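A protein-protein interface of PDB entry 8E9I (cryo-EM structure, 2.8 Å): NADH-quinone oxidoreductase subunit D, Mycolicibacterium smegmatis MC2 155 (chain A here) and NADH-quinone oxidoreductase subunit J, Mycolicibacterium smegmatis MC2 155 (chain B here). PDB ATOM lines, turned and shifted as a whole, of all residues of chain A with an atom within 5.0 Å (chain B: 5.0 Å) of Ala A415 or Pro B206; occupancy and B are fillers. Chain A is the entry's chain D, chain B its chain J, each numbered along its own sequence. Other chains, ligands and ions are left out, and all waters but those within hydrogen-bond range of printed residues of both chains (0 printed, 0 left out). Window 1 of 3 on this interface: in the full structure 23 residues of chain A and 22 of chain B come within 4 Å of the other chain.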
ATOM      1  N   ALA A  70      10.247  16.704  14.034  1.00  0.00           N
ATOM      2  CA  ALA A  70      10.112  16.771  15.488  1.00  0.00           C
ATOM      3  C   ALA A  70      10.561  15.441  16.081  1.00  0.00           C
ATOM      4  O   ALA A  70       9.758  14.530  16.277  1.00  0.00           O
ATOM      5  CB  ALA A  70       8.684  17.094  15.891  1.00  0.00           C
ATOM      6  N   CYS A  72      11.749  13.201  19.237  1.00  0.00           N
ATOM      7  CA  CYS A  72      11.329  13.185  20.629  1.00  0.00           C
ATOM      8  C   CYS A  72      12.363  12.451  21.463  1.00  0.00           C
ATOM      9  O   CYS A  72      12.722  11.313  21.151  1.00  0.00           O
ATOM     10  CB  CYS A  72       9.968  12.522  20.790  1.00  0.00           C
ATOM     11  SG  CYS A  72       9.201  12.862  22.375  1.00  0.00           S
ATOM     12  N   LEU A 411       3.039  10.199  22.853  1.00  0.00           N
ATOM     13  CA  LEU A 411       4.162  11.020  22.427  1.00  0.00           C
ATOM     14  C   LEU A 411       4.728  10.570  21.092  1.00  0.00           C
ATOM     15  O   LEU A 411       5.538  11.293  20.506  1.00  0.00           O
ATOM     16  CB  LEU A 411       5.259  11.016  23.484  1.00  0.00           C
ATOM     17  CG  LEU A 411       5.057  12.005  24.626  1.00  0.00           C
ATOM     18  CD1 LEU A 411       6.229  11.924  25.565  1.00  0.00           C
ATOM     19  CD2 LEU A 411       4.879  13.416  24.118  1.00  0.00           C
ATOM     20  N   GLN A 412       4.328   9.403  20.595  1.00  0.00           N
ATOM     21  CA  GLN A 412       4.661   9.059  19.222  1.00  0.00           C
ATOM     22  C   GLN A 412       3.972   9.994  18.242  1.00  0.00           C
ATOM     23  O   GLN A 412       4.337  10.034  17.063  1.00  0.00           O
ATOM     24  CB  GLN A 412       4.271   7.616  18.934  1.00  0.00           C
ATOM     25  CG  GLN A 412       4.864   6.617  19.897  1.00  0.00           C
ATOM     26  CD  GLN A 412       5.008   5.252  19.284  1.00  0.00           C
ATOM     27  OE1 GLN A 412       4.910   5.091  18.072  1.00  0.00           O
ATOM     28  NE2 GLN A 412       5.221   4.251  20.118  1.00  0.00           N
ATOM     29  N   ALA A 413       2.973  10.743  18.703  1.00  0.00           N
ATOM     30  CA  ALA A 413       2.232  11.645  17.836  1.00  0.00           C
ATOM     31  C   ALA A 413       2.839  13.035  17.757  1.00  0.00           C
ATOM     32  O   ALA A 413       2.268  13.889  17.072  1.00  0.00           O
ATOM     33  CB  ALA A 413       0.787  11.750  18.317  1.00  0.00           C
ATOM     34  N   VAL A 414       3.959  13.302  18.435  1.00  0.00           N
ATOM     35  CA  VAL A 414       4.566  14.624  18.326  1.00  0.00           C
ATOM     36  C   VAL A 414       4.987  14.894  16.893  1.00  0.00           C
ATOM     37  O   VAL A 414       4.794  16.000  16.380  1.00  0.00           O
ATOM     38  CB  VAL A 414       5.759  14.772  19.291  1.00  0.00           C
ATOM     39  CG1 VAL A 414       5.302  14.650  20.729  1.00  0.00           C
ATOM     40  CG2 VAL A 414       6.829  13.749  18.979  1.00  0.00           C
ATOM     41  N   ALA A 415       5.565  13.903  16.221  1.00  0.00           N
ATOM     42  CA  ALA A 415       5.964  14.079  14.832  1.00  0.00           C
ATOM     43  C   ALA A 415       4.760  14.423  13.973  1.00  0.00           C
ATOM     44  O   ALA A 415       4.788  15.393  13.213  1.00  0.00           O
ATOM     45  CB  ALA A 415       6.641  12.819  14.297  1.00  0.00           C
ATOM     46  N   ALA A 416       3.695  13.634  14.098  1.00  0.00           N
ATOM     47  CA  ALA A 416       2.517  13.826  13.264  1.00  0.00           C
ATOM     48  C   ALA A 416       1.866  15.179  13.505  1.00  0.00           C
ATOM     49  O   ALA A 416       1.471  15.867  12.558  1.00  0.00           O
ATOM     50  CB  ALA A 416       1.517  12.702  13.526  1.00  0.00           C
ATOM     51  N   THR A 417       1.747  15.582  14.767  1.00  0.00           N
ATOM     52  CA  THR A 417       0.976  16.773  15.098  1.00  0.00           C
ATOM     53  C   THR A 417       1.807  18.045  15.115  1.00  0.00           C
ATOM     54  O   THR A 417       1.234  19.135  15.205  1.00  0.00           O
ATOM     55  CB  THR A 417       0.306  16.598  16.459  1.00  0.00           C
ATOM     56  OG1 THR A 417       1.301  16.322  17.453  1.00  0.00           O
ATOM     57  CG2 THR A 417      -0.687  15.462  16.414  1.00  0.00           C
ATOM     58  N   CYS A 418       3.131  17.942  15.035  1.00  0.00           N
ATOM     59  CA  CYS A 418       3.988  19.119  15.037  1.00  0.00           C
ATOM     60  C   CYS A 418       4.615  19.397  13.684  1.00  0.00           C
ATOM     61  O   CYS A 418       4.676  20.556  13.268  1.00  0.00           O
ATOM     62  CB  CYS A 418       5.102  18.959  16.074  1.00  0.00           C
ATOM     63  SG  CYS A 418       4.521  18.745  17.769  1.00  0.00           S
ATOM     64  N   GLU A 419       5.062  18.360  12.984  1.00  0.00           N
ATOM     65  CA  GLU A 419       5.756  18.554  11.722  1.00  0.00           C
ATOM     66  C   GLU A 419       4.871  19.315  10.746  1.00  0.00           C
ATOM     67  O   GLU A 419       3.680  19.031  10.608  1.00  0.00           O
ATOM     68  CB  GLU A 419       6.163  17.206  11.133  1.00  0.00           C
ATOM     69  N   THR B 200       4.865  10.841   8.223  1.00  0.00           N
ATOM     70  CA  THR B 200       5.527  11.404   9.396  1.00  0.00           C
ATOM     71  C   THR B 200       5.304  10.592  10.663  1.00  0.00           C
ATOM     72  O   THR B 200       5.953  10.857  11.678  1.00  0.00           O
ATOM     73  CB  THR B 200       5.062  12.842   9.650  1.00  0.00           C
ATOM     74  OG1 THR B 200       3.738  12.826  10.196  1.00  0.00           O
ATOM     75  CG2 THR B 200       5.082  13.666   8.369  1.00  0.00           C
ATOM     76  N   HIS B 203       6.030   6.309   8.917  1.00  0.00           N
ATOM     77  CA  HIS B 203       7.494   6.278   8.692  1.00  0.00           C
ATOM     78  C   HIS B 203       8.144   6.537  10.032  1.00  0.00           C
ATOM     79  O   HIS B 203       7.510   7.252  10.821  1.00  0.00           O
ATOM     80  CB  HIS B 203       7.875   7.272   7.600  1.00  0.00           C
ATOM     81  CG  HIS B 203       7.147   7.008   6.326  1.00  0.00           C
ATOM     82  ND1 HIS B 203       7.379   5.877   5.568  1.00  0.00           N
ATOM     83  CD2 HIS B 203       6.180   7.700   5.687  1.00  0.00           C
ATOM     84  CE1 HIS B 203       6.595   5.892   4.510  1.00  0.00           C
ATOM     85  NE2 HIS B 203       5.850   7.000   4.560  1.00  0.00           N
ATOM     86  N   PRO B 204       9.365   6.035  10.319  1.00  0.00           N
ATOM     87  CA  PRO B 204       9.952   6.119  11.651  1.00  0.00           C
ATOM     88  C   PRO B 204       9.056   6.902  12.623  1.00  0.00           C
ATOM     89  O   PRO B 204       9.500   7.919  13.103  1.00  0.00           O
ATOM     90  CB  PRO B 204      11.232   6.832  11.233  1.00  0.00           C
ATOM     91  CG  PRO B 204      11.643   6.102   9.962  1.00  0.00           C
ATOM     92  CD  PRO B 204      10.364   5.531   9.380  1.00  0.00           C
ATOM     93  N   THR B 205       7.851   6.384  12.911  1.00  0.00           N
ATOM     94  CA  THR B 205       6.880   7.103  13.778  1.00  0.00           C
ATOM     95  C   THR B 205       7.455   8.491  14.017  1.00  0.00           C
ATOM     96  O   THR B 205       7.258   9.336  13.144  1.00  0.00           O
ATOM     97  CB  THR B 205       6.528   6.250  14.999  1.00  0.00           C
ATOM     98  OG1 THR B 205       5.978   5.018  14.539  1.00  0.00           O
ATOM     99  CG2 THR B 205       5.548   6.940  15.921  1.00  0.00           C
ATOM    100  N   PRO B 206       8.169   8.781  15.119  1.00  0.00           N
ATOM    101  CA  PRO B 206       8.835  10.045  15.284  1.00  0.00           C
ATOM    102  C   PRO B 206      10.319   9.694  15.160  1.00  0.00           C
ATOM    103  O   PRO B 206      10.823   8.947  15.963  1.00  0.00           O
ATOM    104  CB  PRO B 206       8.403  10.411  16.703  1.00  0.00           C
ATOM    105  CG  PRO B 206       8.133   9.087  17.396  1.00  0.00           C
ATOM    106  CD  PRO B 206       8.324   8.012  16.346  1.00  0.00           C
ATOM    107  N   LEU B 207      10.989  10.222  14.142  1.00  0.00           N
ATOM    108  CA  LEU B 207      12.398   9.827  13.914  1.00  0.00           C
ATOM    109  C   LEU B 207      13.134   9.720  15.248  1.00  0.00           C
ATOM    110  O   LEU B 207      12.857  10.511  16.153  1.00  0.00           O
ATOM    111  CB  LEU B 207      13.051  10.837  12.972  1.00  0.00           C
ATOM    112  CG  LEU B 207      12.922  10.514  11.487  1.00  0.00           C
ATOM    113  CD1 LEU B 207      13.482  11.646  10.645  1.00  0.00           C
ATOM    114  CD2 LEU B 207      13.634   9.213  11.164  1.00  0.00           C
ATOM    115  N   PRO B 208      14.084   8.786  15.382  1.00  0.00           N
ATOM    116  CA  PRO B 208      14.799   8.525  16.631  1.00  0.00           C
ATOM    117  C   PRO B 208      15.591   9.745  17.073  1.00  0.00           C
ATOM    118  O   PRO B 208      16.138  10.496  16.264  1.00  0.00           O
ATOM    119  CB  PRO B 208      15.722   7.352  16.281  1.00  0.00           C
ATOM    120  CG  PRO B 208      15.798   7.347  14.801  1.00  0.00           C
ATOM    121  CD  PRO B 208      14.486   7.854  14.320  1.00  0.00           C
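The backbone carbonyl oxygen (O) of Thr B205 sits close to the backbone carbonyl oxygen (O) of Thr B200 (2.5 Å).
Gln A412 touches Thr B205 (OE1 to CG2, 2.9 Å). CG of Pro B206 touches CA of Gln A412 (3.9 Å). Ala A415 touches Thr B200. CB of Ala A415 touches O of Thr B205 (3.7 Å). CA of Pro B206 touches CB of Ala A415 (3.7 Å). Ala A416 touches Thr B200.
Of the printed residues of chain B, Gln A412 touches Thr B205 (2.9 Å) and Pro B206 (3.9 Å). Ala A415 touches three residues of chain B. Of the printed residues of chain B, Ala A416 touches Thr B200 (3.5 Å). Cys A418 touches none of the printed residues of chain B. Of the printed residues of chain A, Thr B200 touches Ala A415 (3.3 Å) and Ala A416 (3.5 Å). Pro B204 touches none of the printed residues of chain A. Of the printed residues of chain A, Thr B205 touches Gln A412 (2.9 Å) and Ala A415 (3.7 Å). Pro B206 touches just these residues of chain A: Gln A412 (3.9 Å) and Ala A415 (3.7 Å). The nearest printed residue of chain B that does not touch Ala A415 is Leu B207 (5.1 Å). The nearest printed residue of chain A that does not touch Pro B206 is Val A414 (4.3 Å).
Of the 11 printed residues of chain A, 3 touch a printed residue of chain B. Hydrophobic or aromatic side chains of chain A that line the printed part of chain B: Ala A415. Hydrophobic or aromatic side chains of chain B within 4 Å of the printed part of chain A: Pro B206.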
